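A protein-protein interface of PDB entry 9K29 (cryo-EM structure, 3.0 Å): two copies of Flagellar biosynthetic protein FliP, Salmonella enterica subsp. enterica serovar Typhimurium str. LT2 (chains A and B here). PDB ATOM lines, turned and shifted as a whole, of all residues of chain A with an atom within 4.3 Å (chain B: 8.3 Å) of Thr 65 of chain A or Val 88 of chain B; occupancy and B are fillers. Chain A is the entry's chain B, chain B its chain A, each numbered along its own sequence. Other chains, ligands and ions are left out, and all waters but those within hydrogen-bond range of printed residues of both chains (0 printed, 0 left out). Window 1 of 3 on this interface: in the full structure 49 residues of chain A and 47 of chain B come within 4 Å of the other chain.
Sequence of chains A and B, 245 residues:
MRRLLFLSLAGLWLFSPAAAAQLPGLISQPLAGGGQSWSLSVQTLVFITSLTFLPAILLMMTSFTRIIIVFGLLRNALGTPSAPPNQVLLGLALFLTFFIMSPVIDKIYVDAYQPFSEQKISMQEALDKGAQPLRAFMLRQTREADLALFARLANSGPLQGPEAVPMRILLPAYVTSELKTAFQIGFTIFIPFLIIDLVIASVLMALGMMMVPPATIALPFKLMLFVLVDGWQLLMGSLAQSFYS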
ATOM      1  N   MET A  60      26.441   1.161 -22.611  1.00  0.00           N
ATOM      2  CA  MET A  60      26.150   1.695 -21.287  1.00  0.00           C
ATOM      3  C   MET A  60      26.345   0.657 -20.190  1.00  0.00           C
ATOM      4  O   MET A  60      26.747   1.017 -19.078  1.00  0.00           O
ATOM      5  CB  MET A  60      24.734   2.265 -21.240  1.00  0.00           C
ATOM      6  CG  MET A  60      24.534   3.473 -22.134  1.00  0.00           C
ATOM      7  SD  MET A  60      25.587   4.863 -21.675  1.00  0.00           S
ATOM      8  CE  MET A  60      26.868   4.751 -22.923  1.00  0.00           C
ATOM      9  N   SER A  63      32.162  -0.376 -19.669  1.00  0.00           N
ATOM     10  CA  SER A  63      32.963   0.731 -19.168  1.00  0.00           C
ATOM     11  C   SER A  63      33.180   1.883 -20.142  1.00  0.00           C
ATOM     12  O   SER A  63      34.070   2.711 -19.915  1.00  0.00           O
ATOM     13  CB  SER A  63      34.293   0.182 -18.650  1.00  0.00           C
ATOM     14  OG  SER A  63      35.099  -0.286 -19.716  1.00  0.00           O
ATOM     15  N   PHE A  64      32.397   1.951 -21.219  1.00  0.00           N
ATOM     16  CA  PHE A  64      32.607   2.983 -22.229  1.00  0.00           C
ATOM     17  C   PHE A  64      32.486   4.403 -21.694  1.00  0.00           C
ATOM     18  O   PHE A  64      33.273   5.281 -22.068  1.00  0.00           O
ATOM     19  CB  PHE A  64      31.635   2.767 -23.385  1.00  0.00           C
ATOM     20  CG  PHE A  64      31.944   3.590 -24.600  1.00  0.00           C
ATOM     21  CD1 PHE A  64      33.116   3.394 -25.306  1.00  0.00           C
ATOM     22  CD2 PHE A  64      31.058   4.559 -25.039  1.00  0.00           C
ATOM     23  CE1 PHE A  64      33.402   4.148 -26.425  1.00  0.00           C
ATOM     24  CE2 PHE A  64      31.339   5.317 -26.158  1.00  0.00           C
ATOM     25  CZ  PHE A  64      32.512   5.111 -26.852  1.00  0.00           C
ATOM     26  N   THR A  65      31.503   4.648 -20.823  1.00  0.00           N
ATOM     27  CA  THR A  65      31.168   6.013 -20.427  1.00  0.00           C
ATOM     28  C   THR A  65      32.343   6.707 -19.750  1.00  0.00           C
ATOM     29  O   THR A  65      32.753   7.802 -20.158  1.00  0.00           O
ATOM     30  CB  THR A  65      29.953   5.996 -19.499  1.00  0.00           C
ATOM     31  OG1 THR A  65      28.943   5.138 -20.044  1.00  0.00           O
ATOM     32  CG2 THR A  65      29.391   7.394 -19.326  1.00  0.00           C
ATOM     33  N   ARG A  66      32.904   6.077 -18.716  1.00  0.00           N
ATOM     34  CA  ARG A  66      33.992   6.698 -17.970  1.00  0.00           C
ATOM     35  C   ARG A  66      35.192   6.959 -18.867  1.00  0.00           C
ATOM     36  O   ARG A  66      35.766   8.053 -18.850  1.00  0.00           O
ATOM     37  CB  ARG A  66      34.398   5.810 -16.796  1.00  0.00           C
ATOM     38  CG  ARG A  66      35.445   6.430 -15.890  1.00  0.00           C
ATOM     39  CD  ARG A  66      35.936   5.441 -14.848  1.00  0.00           C
ATOM     40  NE  ARG A  66      34.870   4.993 -13.961  1.00  0.00           N
ATOM     41  CZ  ARG A  66      34.990   4.000 -13.091  1.00  0.00           C
ATOM     42  NH1 ARG A  66      36.122   3.328 -12.963  1.00  0.00           N
ATOM     43  NH2 ARG A  66      33.949   3.674 -12.331  1.00  0.00           N
ATOM     44  N   ILE A  67      35.574   5.964 -19.668  1.00  0.00           N
ATOM     45  CA  ILE A  67      36.766   6.083 -20.501  1.00  0.00           C
ATOM     46  C   ILE A  67      36.593   7.196 -21.527  1.00  0.00           C
ATOM     47  O   ILE A  67      37.475   8.050 -21.698  1.00  0.00           O
ATOM     48  CB  ILE A  67      37.077   4.732 -21.169  1.00  0.00           C
ATOM     49  CG1 ILE A  67      37.716   3.781 -20.156  1.00  0.00           C
ATOM     50  CG2 ILE A  67      37.971   4.917 -22.370  1.00  0.00           C
ATOM     51  CD1 ILE A  67      37.613   2.326 -20.535  1.00  0.00           C
ATOM     52  N   ILE A  68      35.446   7.221 -22.210  1.00  0.00           N
ATOM     53  CA  ILE A  68      35.257   8.207 -23.268  1.00  0.00           C
ATOM     54  C   ILE A  68      35.147   9.611 -22.685  1.00  0.00           C
ATOM     55  O   ILE A  68      35.672  10.572 -23.260  1.00  0.00           O
ATOM     56  CB  ILE A  68      34.041   7.846 -24.145  1.00  0.00           C
ATOM     57  CG1 ILE A  68      34.064   8.669 -25.434  1.00  0.00           C
ATOM     58  CG2 ILE A  68      32.728   8.070 -23.411  1.00  0.00           C
ATOM     59  CD1 ILE A  68      35.030   8.152 -26.471  1.00  0.00           C
ATOM     60  N   ILE A  69      34.497   9.758 -21.527  1.00  0.00           N
ATOM     61  CA  ILE A  69      34.383  11.083 -20.929  1.00  0.00           C
ATOM     62  C   ILE A  69      35.743  11.570 -20.446  1.00  0.00           C
ATOM     63  O   ILE A  69      36.099  12.739 -20.636  1.00  0.00           O
ATOM     64  CB  ILE A  69      33.342  11.075 -19.797  1.00  0.00           C
ATOM     65  CG1 ILE A  69      31.939  10.928 -20.383  1.00  0.00           C
ATOM     66  CG2 ILE A  69      33.433  12.347 -18.973  1.00  0.00           C
ATOM     67  CD1 ILE A  69      30.874  10.746 -19.346  1.00  0.00           C
ATOM     68  N   LEU A 179      29.538   8.455 -14.191  1.00  0.00           N
ATOM     69  CA  LEU A 179      29.658   9.866 -14.541  1.00  0.00           C
ATOM     70  C   LEU A 179      30.451  10.626 -13.486  1.00  0.00           C
ATOM     71  O   LEU A 179      31.337  11.426 -13.817  1.00  0.00           O
ATOM     72  CB  LEU A 179      28.272  10.486 -14.712  1.00  0.00           C
ATOM     73  CG  LEU A 179      27.410   9.986 -15.871  1.00  0.00           C
ATOM     74  CD1 LEU A 179      26.058  10.675 -15.868  1.00  0.00           C
ATOM     75  CD2 LEU A 179      28.112  10.201 -17.193  1.00  0.00           C
ATOM     76  N   ILE B  68      16.840  14.113 -22.216  1.00  0.00           N
ATOM     77  CA  ILE B  68      17.900  14.300 -23.203  1.00  0.00           C
ATOM     78  C   ILE B  68      18.151  15.784 -23.443  1.00  0.00           C
ATOM     79  O   ILE B  68      19.294  16.212 -23.642  1.00  0.00           O
ATOM     80  CB  ILE B  68      17.569  13.547 -24.508  1.00  0.00           C
ATOM     81  CG1 ILE B  68      18.828  13.390 -25.362  1.00  0.00           C
ATOM     82  CG2 ILE B  68      16.478  14.248 -25.302  1.00  0.00           C
ATOM     83  CD1 ILE B  68      19.887  12.520 -24.729  1.00  0.00           C
ATOM     84  N   PHE B  71      20.121  17.170 -20.506  1.00  0.00           N
ATOM     85  CA  PHE B  71      21.514  16.735 -20.549  1.00  0.00           C
ATOM     86  C   PHE B  71      22.285  17.423 -21.671  1.00  0.00           C
ATOM     87  O   PHE B  71      23.473  17.725 -21.518  1.00  0.00           O
ATOM     88  CB  PHE B  71      21.573  15.216 -20.672  1.00  0.00           C
ATOM     89  CG  PHE B  71      21.366  14.510 -19.368  1.00  0.00           C
ATOM     90  CD1 PHE B  71      21.961  14.988 -18.214  1.00  0.00           C
ATOM     91  CD2 PHE B  71      20.544  13.405 -19.280  1.00  0.00           C
ATOM     92  CE1 PHE B  71      21.768  14.355 -17.005  1.00  0.00           C
ATOM     93  CE2 PHE B  71      20.345  12.770 -18.068  1.00  0.00           C
ATOM     94  CZ  PHE B  71      20.958  13.245 -16.933  1.00  0.00           C
ATOM     95  N   ARG B  75      25.557  19.721 -21.307  1.00  0.00           N
ATOM     96  CA  ARG B  75      26.733  19.604 -22.163  1.00  0.00           C
ATOM     97  C   ARG B  75      27.152  20.962 -22.708  1.00  0.00           C
ATOM     98  O   ARG B  75      28.346  21.284 -22.743  1.00  0.00           O
ATOM     99  CB  ARG B  75      26.451  18.635 -23.309  1.00  0.00           C
ATOM    100  CG  ARG B  75      27.601  17.705 -23.636  1.00  0.00           C
ATOM    101  CD  ARG B  75      27.201  16.708 -24.710  1.00  0.00           C
ATOM    102  NE  ARG B  75      26.536  17.358 -25.833  1.00  0.00           N
ATOM    103  CZ  ARG B  75      25.913  16.713 -26.808  1.00  0.00           C
ATOM    104  NH1 ARG B  75      25.855  15.392 -26.836  1.00  0.00           N
ATOM    105  NH2 ARG B  75      25.333  17.410 -27.780  1.00  0.00           N
ATOM    106  N   ALA B  83      31.594  16.481 -25.370  1.00  0.00           N
ATOM    107  CA  ALA B  83      32.584  15.825 -24.517  1.00  0.00           C
ATOM    108  C   ALA B  83      32.117  14.432 -24.119  1.00  0.00           C
ATOM    109  O   ALA B  83      32.910  13.481 -24.239  1.00  0.00           O
ATOM    110  CB  ALA B  83      32.919  16.708 -23.310  1.00  0.00           C
ATOM    111  N   PRO B  84      30.887  14.226 -23.648  1.00  0.00           N
ATOM    112  CA  PRO B  84      30.289  12.900 -23.748  1.00  0.00           C
ATOM    113  C   PRO B  84      29.574  12.752 -25.078  1.00  0.00           C
ATOM    114  O   PRO B  84      28.700  13.565 -25.415  1.00  0.00           O
ATOM    115  CB  PRO B  84      29.306  12.863 -22.570  1.00  0.00           C
ATOM    116  CG  PRO B  84      28.909  14.275 -22.370  1.00  0.00           C
ATOM    117  CD  PRO B  84      30.011  15.156 -22.908  1.00  0.00           C
ATOM    118  N   PRO B  85      29.935  11.747 -25.874  1.00  0.00           N
ATOM    119  CA  PRO B  85      29.326  11.607 -27.204  1.00  0.00           C
ATOM    120  C   PRO B  85      27.817  11.458 -27.116  1.00  0.00           C
ATOM    121  O   PRO B  85      27.260  11.124 -26.068  1.00  0.00           O
ATOM    122  CB  PRO B  85      29.974  10.337 -27.773  1.00  0.00           C
ATOM    123  CG  PRO B  85      31.006   9.900 -26.797  1.00  0.00           C
ATOM    124  CD  PRO B  85      31.113  10.886 -25.689  1.00  0.00           C
ATOM    125  N   ASN B  86      27.151  11.721 -28.244  1.00  0.00           N
ATOM    126  CA  ASN B  86      25.698  11.618 -28.285  1.00  0.00           C
ATOM    127  C   ASN B  86      25.223  10.216 -27.930  1.00  0.00           C
ATOM    128  O   ASN B  86      24.138  10.056 -27.360  1.00  0.00           O
ATOM    129  CB  ASN B  86      25.182  12.020 -29.667  1.00  0.00           C
ATOM    130  CG  ASN B  86      25.183  13.520 -29.873  1.00  0.00           C
ATOM    131  OD1 ASN B  86      25.679  14.273 -29.035  1.00  0.00           O
ATOM    132  ND2 ASN B  86      24.627  13.964 -30.994  1.00  0.00           N
ATOM    133  N   GLN B  87      26.018   9.192 -28.251  1.00  0.00           N
ATOM    134  CA  GLN B  87      25.654   7.829 -27.876  1.00  0.00           C
ATOM    135  C   GLN B  87      25.597   7.667 -26.362  1.00  0.00           C
ATOM    136  O   GLN B  87      24.653   7.070 -25.831  1.00  0.00           O
ATOM    137  CB  GLN B  87      26.643   6.832 -28.481  1.00  0.00           C
ATOM    138  CG  GLN B  87      26.833   6.935 -29.992  1.00  0.00           C
ATOM    139  CD  GLN B  87      25.615   7.483 -30.714  1.00  0.00           C
ATOM    140  OE1 GLN B  87      24.549   6.867 -30.717  1.00  0.00           O
ATOM    141  NE2 GLN B  87      25.770   8.647 -31.336  1.00  0.00           N
ATOM    142  N   VAL B  88      26.595   8.197 -25.651  1.00  0.00           N
ATOM    143  CA  VAL B  88      26.621   8.086 -24.195  1.00  0.00           C
ATOM    144  C   VAL B  88      25.435   8.817 -23.581  1.00  0.00           C
ATOM    145  O   VAL B  88      24.741   8.286 -22.701  1.00  0.00           O
ATOM    146  CB  VAL B  88      27.957   8.620 -23.648  1.00  0.00           C
ATOM    147  CG1 VAL B  88      27.833   8.959 -22.174  1.00  0.00           C
ATOM    148  CG2 VAL B  88      29.065   7.607 -23.876  1.00  0.00           C
ATOM    149  N   LEU B  89      25.185  10.046 -24.037  1.00  0.00           N
ATOM    150  CA  LEU B  89      24.089  10.839 -23.493  1.00  0.00           C
ATOM    151  C   LEU B  89      22.750  10.162 -23.756  1.00  0.00           C
ATOM    152  O   LEU B  89      21.896  10.083 -22.866  1.00  0.00           O
ATOM    153  CB  LEU B  89      24.120  12.242 -24.098  1.00  0.00           C
ATOM    154  CG  LEU B  89      23.609  13.381 -23.219  1.00  0.00           C
ATOM    155  CD1 LEU B  89      24.512  13.543 -22.009  1.00  0.00           C
ATOM    156  CD2 LEU B  89      23.542  14.672 -24.013  1.00  0.00           C
ATOM    157  N   LEU B  90      22.563   9.644 -24.971  1.00  0.00           N
ATOM    158  CA  LEU B  90      21.351   8.919 -25.327  1.00  0.00           C
ATOM    159  C   LEU B  90      21.156   7.655 -24.504  1.00  0.00           C
ATOM    160  O   LEU B  90      20.029   7.388 -24.075  1.00  0.00           O
ATOM    161  CB  LEU B  90      21.383   8.575 -26.817  1.00  0.00           C
ATOM    162  CG  LEU B  90      20.126   7.990 -27.461  1.00  0.00           C
ATOM    163  CD1 LEU B  90      19.920   8.595 -28.836  1.00  0.00           C
ATOM    164  CD2 LEU B  90      20.236   6.479 -27.565  1.00  0.00           C
ATOM    165  N   GLY B  91      22.211   6.878 -24.273  1.00  0.00           N
ATOM    166  CA  GLY B  91      22.095   5.675 -23.474  1.00  0.00           C
ATOM    167  C   GLY B  91      21.763   5.955 -22.025  1.00  0.00           C
ATOM    168  O   GLY B  91      20.916   5.277 -21.430  1.00  0.00           O
ATOM    169  N   LEU B  92      22.417   6.959 -21.439  1.00  0.00           N
ATOM    170  CA  LEU B  92      22.112   7.293 -20.053  1.00  0.00           C
ATOM    171  C   LEU B  92      20.717   7.898 -19.920  1.00  0.00           C
ATOM    172  O   LEU B  92      20.027   7.649 -18.922  1.00  0.00           O
ATOM    173  CB  LEU B  92      23.194   8.214 -19.483  1.00  0.00           C
ATOM    174  CG  LEU B  92      23.492   9.595 -20.067  1.00  0.00           C
ATOM    175  CD1 LEU B  92      22.563  10.642 -19.512  1.00  0.00           C
ATOM    176  CD2 LEU B  92      24.942   9.976 -19.805  1.00  0.00           C
ATOM    177  N   ALA B  93      20.269   8.661 -20.922  1.00  0.00           N
ATOM    178  CA  ALA B  93      18.890   9.135 -20.925  1.00  0.00           C
ATOM    179  C   ALA B  93      17.910   7.972 -21.003  1.00  0.00           C
ATOM    180  O   ALA B  93      16.877   7.974 -20.322  1.00  0.00           O
ATOM    181  CB  ALA B  93      18.670  10.101 -22.088  1.00  0.00           C
ATOM    182  N   LEU B  94      18.215   6.970 -21.831  1.00  0.00           N
ATOM    183  CA  LEU B  94      17.351   5.797 -21.923  1.00  0.00           C
ATOM    184  C   LEU B  94      17.284   5.063 -20.592  1.00  0.00           C
ATOM    185  O   LEU B  94      16.214   4.608 -20.175  1.00  0.00           O
ATOM    186  CB  LEU B  94      17.844   4.858 -23.024  1.00  0.00           C
ATOM    187  CG  LEU B  94      17.605   5.284 -24.471  1.00  0.00           C
ATOM    188  CD1 LEU B  94      18.279   4.308 -25.419  1.00  0.00           C
ATOM    189  CD2 LEU B  94      16.120   5.375 -24.758  1.00  0.00           C
ATOM    190  N   PHE B  95      18.424   4.928 -19.914  1.00  0.00           N
ATOM    191  CA  PHE B  95      18.427   4.262 -18.614  1.00  0.00           C
ATOM    192  C   PHE B  95      17.607   5.040 -17.592  1.00  0.00           C
ATOM    193  O   PHE B  95      16.841   4.451 -16.817  1.00  0.00           O
ATOM    194  CB  PHE B  95      19.857   4.068 -18.119  1.00  0.00           C
ATOM    195  CG  PHE B  95      20.544   2.882 -18.721  1.00  0.00           C
ATOM    196  CD1 PHE B  95      19.903   2.101 -19.666  1.00  0.00           C
ATOM    197  CD2 PHE B  95      21.822   2.534 -18.329  1.00  0.00           C
ATOM    198  CE1 PHE B  95      20.531   1.008 -20.218  1.00  0.00           C
ATOM    199  CE2 PHE B  95      22.452   1.440 -18.874  1.00  0.00           C
ATOM    200  CZ  PHE B  95      21.807   0.677 -19.822  1.00  0.00           C
ATOM    201  N   TRP B 232      25.921  15.372 -10.188  1.00  0.00           N
ATOM    202  CA  TRP B 232      25.281  14.281 -10.916  1.00  0.00           C
ATOM    203  C   TRP B 232      24.145  13.675 -10.102  1.00  0.00           C
ATOM    204  O   TRP B 232      23.040  13.463 -10.616  1.00  0.00           O
ATOM    205  CB  TRP B 232      26.315  13.217 -11.281  1.00  0.00           C
ATOM    206  CG  TRP B 232      27.101  13.541 -12.512  1.00  0.00           C
ATOM    207  CD1 TRP B 232      28.457  13.642 -12.614  1.00  0.00           C
ATOM    208  CD2 TRP B 232      26.580  13.802 -13.822  1.00  0.00           C
ATOM    209  NE1 TRP B 232      28.813  13.954 -13.902  1.00  0.00           N
ATOM    210  CE2 TRP B 232      27.679  14.056 -14.664  1.00  0.00           C
ATOM    211  CE3 TRP B 232      25.292  13.846 -14.362  1.00  0.00           C
ATOM    212  CZ2 TRP B 232      27.529  14.350 -16.017  1.00  0.00           C
ATOM    213  CZ3 TRP B 232      25.145  14.139 -15.705  1.00  0.00           C
ATOM    214  CH2 TRP B 232      26.258  14.386 -16.517  1.00  0.00           C
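The side-chain sulfur (SD) of Met 60 of chain A lies close to the backbone carbonyl oxygen (O) of Val 88 of chain B (3.7 Å).
SD of Met 60 of chain A lies close to OG1 of Thr 65 of chain A (3.7 Å).
Among the printed residues, merely in contact across the chains: Met 60 of chain A with Phe 95 of chain B (3.4 Å), Met 60 of chain A with Gly 91 of chain B (3.5 Å), Ile 68 of chain A with Pro 85 of chain B (3.6 Å), Leu 179 of chain A with Trp 232 of chain B (3.6 Å), Thr 65 of chain A with Val 88 of chain B (3.6 Å), Ile 68 of chain A with Val 88 of chain B (3.7 Å), Met 60 of chain A with Leu 92 of chain B (3.8 Å), Phe 64 of chain A with Val 88 of chain B (3.8 Å) and Ile 69 of chain A with Pro 84 of chain B (3.9 Å).
Printed residues of chain B within 4 Å of Phe 64 of chain A: Val 88 (3.8 Å). Of chain B, only Val 88 (3.6 Å) comes within 4 Å of Thr 65 of chain A. Arg 66 of chain A touches none of the printed residues of chain B. Arg 75 of chain B touches none of the printed residues of chain A. Of the printed residues of chain A, Val 88 of chain B touches Met 60 (3.6 Å), Phe 64 (3.8 Å), Thr 65 (3.6 Å) and Ile 68 (3.7 Å). Of the printed residues of chain A, Leu 92 of chain B touches Met 60 (3.8 Å). Of the printed residues of chain A, Phe 95 of chain B touches Met 60. The nearest printed residue of chain A that does not touch Val 88 of chain B is Ile 69 of chain A (4.5 Å).
Printed residues of chain B that touch a printed residue of chain A: Pro 84, Pro 85, Val 88, Gly 91, Leu 92, Phe 95 and Trp 232. Along chain B the printed residues that touch a printed residue of chain A span positions 84 to 232. Of the 9 printed residues of chain A, 6 touch a printed residue of chain B. Among the printed residues, 10 pairs touch across the chains. Among the printed residues, no Asp or Glu carboxylate lies within 4 Å of a Lys or Arg side-chain nitrogen of the other chain.
Position printed for both chains: 68. Of the 10 pairs that touch across the chains among the printed residues, none has its exchanged pair printed and touching as well.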
